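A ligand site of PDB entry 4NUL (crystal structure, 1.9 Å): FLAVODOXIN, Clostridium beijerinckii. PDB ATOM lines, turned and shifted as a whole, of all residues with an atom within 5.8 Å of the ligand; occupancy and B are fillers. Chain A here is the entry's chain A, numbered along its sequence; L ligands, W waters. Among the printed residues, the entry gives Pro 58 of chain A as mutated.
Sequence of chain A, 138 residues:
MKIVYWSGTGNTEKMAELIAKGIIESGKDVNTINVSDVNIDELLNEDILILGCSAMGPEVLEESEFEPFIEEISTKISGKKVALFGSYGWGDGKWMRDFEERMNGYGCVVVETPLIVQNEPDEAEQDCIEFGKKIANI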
ATOM      1  N   TRP A   6      -7.283  16.858  -8.164  1.00  0.00           N
ATOM      2  CA  TRP A   6      -7.253  15.553  -8.794  1.00  0.00           C
ATOM      3  C   TRP A   6      -6.505  14.684  -7.783  1.00  0.00           C
ATOM      4  O   TRP A   6      -5.516  15.144  -7.190  1.00  0.00           O
ATOM      5  CB  TRP A   6      -6.488  15.542 -10.139  1.00  0.00           C
ATOM      6  CG  TRP A   6      -6.573  14.177 -10.796  1.00  0.00           C
ATOM      7  CD1 TRP A   6      -7.577  13.724 -11.617  1.00  0.00           C
ATOM      8  CD2 TRP A   6      -5.702  13.055 -10.588  1.00  0.00           C
ATOM      9  NE1 TRP A   6      -7.388  12.393 -11.907  1.00  0.00           N
ATOM     10  CE2 TRP A   6      -6.242  11.962 -11.295  1.00  0.00           C
ATOM     11  CE3 TRP A   6      -4.501  12.873  -9.862  1.00  0.00           C
ATOM     12  CZ2 TRP A   6      -5.627  10.687 -11.302  1.00  0.00           C
ATOM     13  CZ3 TRP A   6      -3.892  11.604  -9.882  1.00  0.00           C
ATOM     14  CH2 TRP A   6      -4.469  10.542 -10.598  1.00  0.00           C
ATOM     15  N   SER A   7      -6.970  13.454  -7.573  1.00  0.00           N
ATOM     16  CA  SER A   7      -6.329  12.518  -6.638  1.00  0.00           C
ATOM     17  C   SER A   7      -6.519  11.103  -7.169  1.00  0.00           C
ATOM     18  O   SER A   7      -7.639  10.699  -7.534  1.00  0.00           O
ATOM     19  CB  SER A   7      -6.937  12.658  -5.251  1.00  0.00           C
ATOM     20  OG  SER A   7      -6.311  11.802  -4.299  1.00  0.00           O
ATOM     21  N   GLY A   8      -5.426  10.339  -7.219  1.00  0.00           N
ATOM     22  CA  GLY A   8      -5.471   8.983  -7.740  1.00  0.00           C
ATOM     23  C   GLY A   8      -5.727   7.912  -6.700  1.00  0.00           C
ATOM     24  O   GLY A   8      -6.282   6.869  -7.018  1.00  0.00           O
ATOM     25  N   THR A   9      -5.263   8.135  -5.478  1.00  0.00           N
ATOM     26  CA  THR A   9      -5.493   7.163  -4.408  1.00  0.00           C
ATOM     27  C   THR A   9      -6.190   7.807  -3.209  1.00  0.00           C
ATOM     28  O   THR A   9      -6.562   7.119  -2.250  1.00  0.00           O
ATOM     29  CB  THR A   9      -4.181   6.459  -3.948  1.00  0.00           C
ATOM     30  OG1 THR A   9      -3.405   7.343  -3.139  1.00  0.00           O
ATOM     31  CG2 THR A   9      -3.368   5.993  -5.148  1.00  0.00           C
ATOM     32  N   GLY A  10      -6.353   9.119  -3.239  1.00  0.00           N
ATOM     33  CA  GLY A  10      -7.039   9.803  -2.156  1.00  0.00           C
ATOM     34  C   GLY A  10      -6.180  10.643  -1.237  1.00  0.00           C
ATOM     35  O   GLY A  10      -6.706  11.235  -0.293  1.00  0.00           O
ATOM     36  N   ASN A  11      -4.884  10.725  -1.485  1.00  0.00           N
ATOM     37  CA  ASN A  11      -4.007  11.521  -0.630  1.00  0.00           C
ATOM     38  C   ASN A  11      -4.259  13.017  -0.790  1.00  0.00           C
ATOM     39  O   ASN A  11      -4.457  13.719   0.212  1.00  0.00           O
ATOM     40  CB  ASN A  11      -2.532  11.189  -0.885  1.00  0.00           C
ATOM     41  CG  ASN A  11      -2.193   9.783  -0.441  1.00  0.00           C
ATOM     42  OD1 ASN A  11      -1.218   9.181  -0.896  1.00  0.00           O
ATOM     43  ND2 ASN A  11      -3.008   9.249   0.447  1.00  0.00           N
ATOM     44  N   THR A  12      -4.287  13.478  -2.033  1.00  0.00           N
ATOM     45  CA  THR A  12      -4.553  14.888  -2.326  1.00  0.00           C
ATOM     46  C   THR A  12      -5.999  15.238  -1.967  1.00  0.00           C
ATOM     47  O   THR A  12      -6.281  16.361  -1.557  1.00  0.00           O
ATOM     48  CB  THR A  12      -4.258  15.227  -3.814  1.00  0.00           C
ATOM     49  OG1 THR A  12      -2.875  14.921  -4.096  1.00  0.00           O
ATOM     50  CG2 THR A  12      -4.454  16.709  -4.078  1.00  0.00           C
ATOM     51  N   GLU A  13      -6.894  14.264  -2.106  1.00  0.00           N
ATOM     52  CA  GLU A  13      -8.305  14.462  -1.772  1.00  0.00           C
ATOM     53  C   GLU A  13      -8.457  14.734  -0.272  1.00  0.00           C
ATOM     54  O   GLU A  13      -9.223  15.631   0.127  1.00  0.00           O
ATOM     55  CB  GLU A  13      -9.141  13.253  -2.154  1.00  0.00           C
ATOM     56  CG  GLU A  13     -10.586  13.416  -1.757  1.00  0.00           C
ATOM     57  CD  GLU A  13     -11.485  12.287  -2.251  1.00  0.00           C
ATOM     58  OE1 GLU A  13     -11.005  11.154  -2.460  1.00  0.00           O
ATOM     59  OE2 GLU A  13     -12.689  12.554  -2.419  1.00  0.00           O
ATOM     60  N   SER A  54      -1.592  15.633  -7.201  1.00  0.00           N
ATOM     61  CA  SER A  54      -0.435  14.851  -6.780  1.00  0.00           C
ATOM     62  C   SER A  54       0.631  14.807  -7.876  1.00  0.00           C
ATOM     63  O   SER A  54       0.370  15.169  -9.034  1.00  0.00           O
ATOM     64  CB  SER A  54      -0.886  13.425  -6.458  1.00  0.00           C
ATOM     65  OG  SER A  54      -1.639  12.901  -7.541  1.00  0.00           O
ATOM     66  N   ALA A  55       1.828  14.364  -7.500  1.00  0.00           N
ATOM     67  CA  ALA A  55       2.935  14.274  -8.441  1.00  0.00           C
ATOM     68  C   ALA A  55       2.831  13.027  -9.302  1.00  0.00           C
ATOM     69  O   ALA A  55       2.834  11.912  -8.771  1.00  0.00           O
ATOM     70  CB  ALA A  55       4.261  14.290  -7.677  1.00  0.00           C
ATOM     71  N   MET A  56       2.636  13.205 -10.607  1.00  0.00           N
ATOM     72  CA  MET A  56       2.583  12.073 -11.529  1.00  0.00           C
ATOM     73  C   MET A  56       3.939  11.981 -12.233  1.00  0.00           C
ATOM     74  O   MET A  56       4.805  12.836 -12.019  1.00  0.00           O
ATOM     75  CB  MET A  56       1.411  12.181 -12.515  1.00  0.00           C
ATOM     76  CG  MET A  56       0.043  11.866 -11.896  1.00  0.00           C
ATOM     77  SD  MET A  56      -0.109  10.198 -11.142  1.00  0.00           S
ATOM     78  CE  MET A  56      -0.045  10.618  -9.391  1.00  0.00           C
ATOM     79  N   GLY A  57       4.150  10.951 -13.043  1.00  0.00           N
ATOM     80  CA  GLY A  57       5.465  10.765 -13.647  1.00  0.00           C
ATOM     81  C   GLY A  57       5.708  11.286 -15.047  1.00  0.00           C
ATOM     82  O   GLY A  57       4.837  11.156 -15.907  1.00  0.00           O
ATOM     83  N   PRO A  58       6.885  11.877 -15.304  1.00  0.00           N
ATOM     84  CA  PRO A  58       7.989  12.097 -14.354  1.00  0.00           C
ATOM     85  C   PRO A  58       7.936  13.516 -13.763  1.00  0.00           C
ATOM     86  O   PRO A  58       8.297  14.476 -14.437  1.00  0.00           O
ATOM     87  CB  PRO A  58       9.223  11.922 -15.235  1.00  0.00           C
ATOM     88  CG  PRO A  58       8.777  12.539 -16.536  1.00  0.00           C
ATOM     89  CD  PRO A  58       7.323  12.144 -16.691  1.00  0.00           C
ATOM     90  N   GLU A  59       7.504  13.629 -12.512  1.00  0.00           N
ATOM     91  CA  GLU A  59       7.376  14.930 -11.832  1.00  0.00           C
ATOM     92  C   GLU A  59       6.542  15.908 -12.667  1.00  0.00           C
ATOM     93  O   GLU A  59       7.003  17.002 -13.011  1.00  0.00           O
ATOM     94  CB  GLU A  59       8.739  15.558 -11.530  1.00  0.00           C
ATOM     95  CG  GLU A  59       9.579  14.794 -10.512  1.00  0.00           C
ATOM     96  CD  GLU A  59       9.002  14.773  -9.107  1.00  0.00           C
ATOM     97  OE1 GLU A  59       8.225  15.679  -8.741  1.00  0.00           O
ATOM     98  OE2 GLU A  59       9.374  13.871  -8.335  1.00  0.00           O
ATOM     99  N   VAL A  60       5.313  15.509 -12.965  1.00  0.00           N
ATOM    100  CA  VAL A  60       4.413  16.332 -13.765  1.00  0.00           C
ATOM    101  C   VAL A  60       3.009  16.289 -13.180  1.00  0.00           C
ATOM    102  O   VAL A  60       2.689  15.458 -12.326  1.00  0.00           O
ATOM    103  CB  VAL A  60       4.326  15.819 -15.220  1.00  0.00           C
ATOM    104  CG1 VAL A  60       5.637  16.021 -15.953  1.00  0.00           C
ATOM    105  CG2 VAL A  60       3.927  14.337 -15.230  1.00  0.00           C
ATOM    106  N   SER A  87      -0.025  16.029  -2.903  1.00  0.00           N
ATOM    107  CA  SER A  87       0.732  14.966  -2.270  1.00  0.00           C
ATOM    108  C   SER A  87       1.755  14.426  -3.268  1.00  0.00           C
ATOM    109  O   SER A  87       1.531  14.445  -4.483  1.00  0.00           O
ATOM    110  CB  SER A  87      -0.201  13.827  -1.839  1.00  0.00           C
ATOM    111  OG  SER A  87       0.503  12.842  -1.102  1.00  0.00           O
ATOM    112  N   TYR A  88       2.882  13.942  -2.763  1.00  0.00           N
ATOM    113  CA  TYR A  88       3.910  13.388  -3.626  1.00  0.00           C
ATOM    114  C   TYR A  88       4.460  12.150  -2.944  1.00  0.00           C
ATOM    115  O   TYR A  88       4.162  11.899  -1.775  1.00  0.00           O
ATOM    116  CB  TYR A  88       4.999  14.418  -3.928  1.00  0.00           C
ATOM    117  CG  TYR A  88       5.818  14.806  -2.725  1.00  0.00           C
ATOM    118  CD1 TYR A  88       5.321  15.719  -1.793  1.00  0.00           C
ATOM    119  CD2 TYR A  88       7.084  14.270  -2.509  1.00  0.00           C
ATOM    120  CE1 TYR A  88       6.054  16.088  -0.690  1.00  0.00           C
ATOM    121  CE2 TYR A  88       7.824  14.632  -1.404  1.00  0.00           C
ATOM    122  CZ  TYR A  88       7.302  15.541  -0.495  1.00  0.00           C
ATOM    123  OH  TYR A  88       8.035  15.909   0.608  1.00  0.00           O
ATOM    124  N   GLY A  89       5.283  11.395  -3.652  1.00  0.00           N
ATOM    125  CA  GLY A  89       5.791  10.150  -3.097  1.00  0.00           C
ATOM    126  C   GLY A  89       7.262  10.158  -2.812  1.00  0.00           C
ATOM    127  O   GLY A  89       7.681  10.564  -1.735  1.00  0.00           O
ATOM    128  N   TRP A  90       8.045   9.778  -3.814  1.00  0.00           N
ATOM    129  CA  TRP A  90       9.501   9.660  -3.686  1.00  0.00           C
ATOM    130  C   TRP A  90      10.353  10.873  -4.077  1.00  0.00           C
ATOM    131  O   TRP A  90      11.553  10.895  -3.799  1.00  0.00           O
ATOM    132  CB  TRP A  90       9.980   8.432  -4.472  1.00  0.00           C
ATOM    133  CG  TRP A  90       9.554   8.464  -5.909  1.00  0.00           C
ATOM    134  CD1 TRP A  90      10.173   9.102  -6.940  1.00  0.00           C
ATOM    135  CD2 TRP A  90       8.404   7.813  -6.476  1.00  0.00           C
ATOM    136  NE1 TRP A  90       9.488   8.890  -8.111  1.00  0.00           N
ATOM    137  CE2 TRP A  90       8.396   8.103  -7.855  1.00  0.00           C
ATOM    138  CE3 TRP A  90       7.372   7.019  -5.956  1.00  0.00           C
ATOM    139  CZ2 TRP A  90       7.413   7.630  -8.721  1.00  0.00           C
ATOM    140  CZ3 TRP A  90       6.389   6.545  -6.822  1.00  0.00           C
ATOM    141  CH2 TRP A  90       6.422   6.854  -8.188  1.00  0.00           C
ATOM    142  N   GLY A  91       9.754  11.860  -4.739  1.00  0.00           N
ATOM    143  CA  GLY A  91      10.528  13.022  -5.163  1.00  0.00           C
ATOM    144  C   GLY A  91      10.703  14.050  -4.067  1.00  0.00           C
ATOM    145  O   GLY A  91      10.470  13.768  -2.885  1.00  0.00           O
ATOM    146  N   ASP A  92      11.118  15.251  -4.443  1.00  0.00           N
ATOM    147  CA  ASP A  92      11.297  16.326  -3.465  1.00  0.00           C
ATOM    148  C   ASP A  92      10.532  17.605  -3.805  1.00  0.00           C
ATOM    149  O   ASP A  92      10.932  18.694  -3.412  1.00  0.00           O
ATOM    150  CB  ASP A  92      12.792  16.606  -3.227  1.00  0.00           C
ATOM    151  CG  ASP A  92      13.523  17.125  -4.470  1.00  0.00           C
ATOM    152  OD1 ASP A  92      12.869  17.576  -5.438  1.00  0.00           O
ATOM    153  OD2 ASP A  92      14.767  17.086  -4.463  1.00  0.00           O
ATOM    154  N   TRP A  95       7.678  18.638  -9.216  1.00  0.00           N
ATOM    155  CA  TRP A  95       6.435  18.898  -9.938  1.00  0.00           C
ATOM    156  C   TRP A  95       5.751  20.168  -9.420  1.00  0.00           C
ATOM    157  O   TRP A  95       5.153  20.910 -10.189  1.00  0.00           O
ATOM    158  CB  TRP A  95       5.489  17.678  -9.885  1.00  0.00           C
ATOM    159  CG  TRP A  95       4.301  17.775  -8.925  1.00  0.00           C
ATOM    160  CD1 TRP A  95       2.977  17.903  -9.262  1.00  0.00           C
ATOM    161  CD2 TRP A  95       4.336  17.717  -7.485  1.00  0.00           C
ATOM    162  NE1 TRP A  95       2.194  17.924  -8.125  1.00  0.00           N
ATOM    163  CE2 TRP A  95       3.009  17.816  -7.023  1.00  0.00           C
ATOM    164  CE3 TRP A  95       5.371  17.595  -6.545  1.00  0.00           C
ATOM    165  CZ2 TRP A  95       2.672  17.794  -5.658  1.00  0.00           C
ATOM    166  CZ3 TRP A  95       5.049  17.572  -5.188  1.00  0.00           C
ATOM    167  CH2 TRP A  95       3.705  17.673  -4.759  1.00  0.00           C
ATOM    168  N   VAL A 117       2.729  17.505   0.732  1.00  0.00           N
ATOM    169  CA  VAL A 117       2.801  16.518   1.793  1.00  0.00           C
ATOM    170  C   VAL A 117       3.145  15.185   1.167  1.00  0.00           C
ATOM    171  O   VAL A 117       2.649  14.861   0.089  1.00  0.00           O
ATOM    172  CB  VAL A 117       1.434  16.392   2.528  1.00  0.00           C
ATOM    173  CG1 VAL A 117       1.421  15.195   3.465  1.00  0.00           C
ATOM    174  CG2 VAL A 117       1.138  17.671   3.310  1.00  0.00           C
ATOM    175  N   GLN A 118       4.008  14.432   1.820  1.00  0.00           N
ATOM    176  CA  GLN A 118       4.402  13.139   1.297  1.00  0.00           C
ATOM    177  C   GLN A 118       3.375  12.095   1.681  1.00  0.00           C
ATOM    178  O   GLN A 118       3.078  11.912   2.871  1.00  0.00           O
ATOM    179  CB  GLN A 118       5.769  12.750   1.830  1.00  0.00           C
ATOM    180  CG  GLN A 118       6.352  11.513   1.191  1.00  0.00           C
ATOM    181  CD  GLN A 118       7.710  11.173   1.768  1.00  0.00           C
ATOM    182  OE1 GLN A 118       7.939  11.324   2.968  1.00  0.00           O
ATOM    183  NE2 GLN A 118       8.610  10.706   0.915  1.00  0.00           N
ATOM    184  N   ASN A 119       2.822  11.435   0.674  1.00  0.00           N
ATOM    185  CA  ASN A 119       1.819  10.392   0.867  1.00  0.00           C
ATOM    186  C   ASN A 119       0.587  10.950   1.581  1.00  0.00           C
ATOM    187  O   ASN A 119       0.228  12.097   1.376  1.00  0.00           O
ATOM    188  CB  ASN A 119       2.433   9.219   1.620  1.00  0.00           C
ATOM    189  CG  ASN A 119       3.729   8.753   0.973  1.00  0.00           C
ATOM    190  OD1 ASN A 119       3.776   8.409  -0.214  1.00  0.00           O
ATOM    191  ND2 ASN A 119       4.823   8.816   1.740  1.00  0.00           N
ATOM    192  N   GLU A 120      -0.067  10.135   2.409  1.00  0.00           N
ATOM    193  CA  GLU A 120      -1.268  10.612   3.097  1.00  0.00           C
ATOM    194  C   GLU A 120      -0.912  11.612   4.190  1.00  0.00           C
ATOM    195  O   GLU A 120       0.099  11.451   4.878  1.00  0.00           O
ATOM    196  CB  GLU A 120      -2.025   9.427   3.690  1.00  0.00           C
ATOM    197  CG  GLU A 120      -3.484   9.719   3.954  1.00  0.00           C
ATOM    198  CD  GLU A 120      -4.227   8.535   4.549  1.00  0.00           C
ATOM    199  OE1 GLU A 120      -4.104   7.416   3.984  1.00  0.00           O
ATOM    200  OE2 GLU A 120      -4.935   8.726   5.558  1.00  0.00           O
HETATM  201  N1  LIG L   1       5.711  10.887  -6.640  1.00  0.00           N
HETATM  202  C1  LIG L   1       6.758  11.693  -6.762  1.00  0.00           C
HETATM  203  O1  LIG L   1       7.224  12.202  -5.776  1.00  0.00           O
HETATM  204  N2  LIG L   1       7.342  11.900  -8.030  1.00  0.00           N
HETATM  205  C2  LIG L   1       6.924  11.354  -9.218  1.00  0.00           C
HETATM  206  O2  LIG L   1       7.466  11.618 -10.286  1.00  0.00           O
HETATM  207  C3  LIG L   1       5.776  10.453  -9.086  1.00  0.00           C
HETATM  208  N3  LIG L   1       5.329   9.803 -10.150  1.00  0.00           N
HETATM  209  C4  LIG L   1       4.301   8.929  -9.965  1.00  0.00           C
HETATM  210  C5  LIG L   1       3.806   8.214 -11.068  1.00  0.00           C
HETATM  211  C6  LIG L   1       2.748   7.392 -10.955  1.00  0.00           C
HETATM  212  C7  LIG L   1       2.282   6.582 -12.131  1.00  0.00           C
HETATM  213  C8  LIG L   1       2.104   7.251  -9.705  1.00  0.00           C
HETATM  214  C9  LIG L   1       0.960   6.307  -9.524  1.00  0.00           C
HETATM  215  C10 LIG L   1       2.573   7.937  -8.601  1.00  0.00           C
HETATM  216  C11 LIG L   1       3.664   8.769  -8.701  1.00  0.00           C
HETATM  217  N4  LIG L   1       4.197   9.424  -7.584  1.00  0.00           N
HETATM  218  C12 LIG L   1       5.240  10.299  -7.717  1.00  0.00           C
HETATM  219  C13 LIG L   1       3.648   9.134  -6.259  1.00  0.00           C
HETATM  220  C14 LIG L   1       2.404   9.960  -5.943  1.00  0.00           C
HETATM  221  O3  LIG L   1       2.645  11.349  -6.166  1.00  0.00           O
HETATM  222  C15 LIG L   1       2.018   9.756  -4.487  1.00  0.00           C
HETATM  223  O4  LIG L   1       1.685   8.382  -4.279  1.00  0.00           O
HETATM  224  C16 LIG L   1       0.881  10.639  -3.971  1.00  0.00           C
HETATM  225  O5  LIG L   1       0.678  10.390  -2.586  1.00  0.00           O
HETATM  226  C17 LIG L   1      -0.414  10.341  -4.711  1.00  0.00           C
HETATM  227  O6  LIG L   1      -1.464  11.107  -4.197  1.00  0.00           O
HETATM  228  P1  LIG L   1      -2.978  10.905  -4.664  1.00  0.00           P
HETATM  229  O7  LIG L   1      -3.588   9.749  -4.066  1.00  0.00           O
HETATM  230  O8  LIG L   1      -3.637  12.212  -4.433  1.00  0.00           O
HETATM  231  O9  LIG L   1      -2.876  10.745  -6.166  1.00  0.00           O
HETATM  232  O   HOH W   1       7.976  15.418  -5.923  1.00  0.00           O
HETATM  233  O   HOH W   2       7.970   8.925 -12.282  1.00  0.00           O
HETATM  234  O   HOH W   3      -2.183   8.412  -7.455  1.00  0.00           O
HETATM  235  O   HOH W   4      -0.109   7.250  -6.155  1.00  0.00           O
HETATM  236  O   HOH W   5       1.641   7.554  -1.666  1.00  0.00           O
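An oxygen (O2) of the ligand sits at hydrogen-bond distance from the backbone NH (N) of Glu 59, 3.0 Å away. An oxygen (O7) of the ligand is in hydrogen-bond range of the backbone NH of Thr 9 (2.7 Å). OG1 of Thr 9 sits at hydrogen-bond distance from O7 of the ligand, at 2.6 Å. The side-chain hydroxyl (OG) of Ser 54 lies within hydrogen-bond range of an oxygen (O9) of the ligand, at 2.8 Å. A nitrogen (N3) of the ligand is in hydrogen-bond range of the backbone NH of Gly 57, 3.3 Å away. The side-chain hydroxyl (OG) of Ser 7 is in hydrogen-bond range of an oxygen (O8) of the ligand, at 2.7 Å. An oxygen (O5) of the ligand lies within hydrogen-bond range of the side-chain hydroxyl (OG) of Ser 87, at 2.9 Å. O7 of the ligand sits at hydrogen-bond distance from N of Asn 11 (3.0 Å). N of Thr 12 sits at hydrogen-bond distance from O8 of the ligand, 2.8 Å away. N of Ala 55 is in hydrogen-bond range of O3 of the ligand. The backbone NH (N) of Gly 89 is in hydrogen-bond range of an oxygen (O1) of the ligand (3.0 Å). An oxygen (O8) of the ligand lies within hydrogen-bond range of the side-chain hydroxyl of Thr 12, 2.8 Å away. N2 of the ligand is in hydrogen-bond range of OE2 of Glu 59, at 2.8 Å. The backbone NH (N) of Trp 90 sits at hydrogen-bond distance from an oxygen (O1) of the ligand (3.2 Å). The backbone NH (N) of Gly 10 sits at hydrogen-bond distance from an oxygen (O7) of the ligand (3.0 Å). The side-chain amide oxygen (OD1) of Asn 11 lies within hydrogen-bond range of an oxygen (O5) of the ligand, at 2.8 Å. O1 of the ligand lies within hydrogen-bond range of N of Gly 91, 2.8 Å away. The backbone NH (N) of Gly 8 is in hydrogen-bond range of an oxygen (O9) of the ligand, at 2.8 Å. The backbone carbonyl oxygen (O) of Ala 55 is in hydrogen-bond range of an oxygen (O3) of the ligand, 2.7 Å away.
Water W5 lies within hydrogen-bond range of OD1 of Asn 119, O4 of the ligand and OD1 of Asn 11. Water W1 lies within hydrogen-bond range of OE1 of Glu 59 (2.8 Å), O1 of the ligand (3.3 Å) and N of Asp 92 (3.5 Å).
NE2 of Gln 118 is in hydrogen-bond range of O of Gly 89, at 2.8 Å. The backbone carbonyl oxygen of Ser 54 sits at hydrogen-bond distance from the indole nitrogen of Trp 95, at 3.4 Å. The side-chain hydroxyl (OG) of Ser 7 is in hydrogen-bond range of the backbone NH (N) of Asn 11. The side-chain hydroxyl (OG) of Ser 7 is in hydrogen-bond range of the backbone NH (N) of Thr 12, 3.5 Å away. The side-chain hydroxyl of Ser 87 is in hydrogen-bond range of the backbone carbonyl oxygen of Asn 119 (2.6 Å). N of Tyr 88 lies within hydrogen-bond range of O of Val 117, 3.0 Å away. The backbone NH (N) of Trp 95 is in hydrogen-bond range of the side-chain carboxylate (OE1) of Glu 59, at 3.0 Å. OG of Ser 7 is in hydrogen-bond range of N of Gly 10, at 2.9 Å.
The backbone carbonyl oxygen (O) of Met 56 sits close to an oxygen (O2) of the ligand (3.4 Å). Merely in contact with the ligand: Trp 6, Pro 58, Tyr 88 and Asn 119. 19 residues have an atom within 4 Å of the ligand: Trp 6, Ser 7, Gly 8, Thr 9, Gly 10, Asn 11, Thr 12, Ser 54, Ala 55, Met 56, Gly 57, Pro 58, Glu 59, Ser 87, Tyr 88, Gly 89, Trp 90, Gly 91 and Asn 119.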
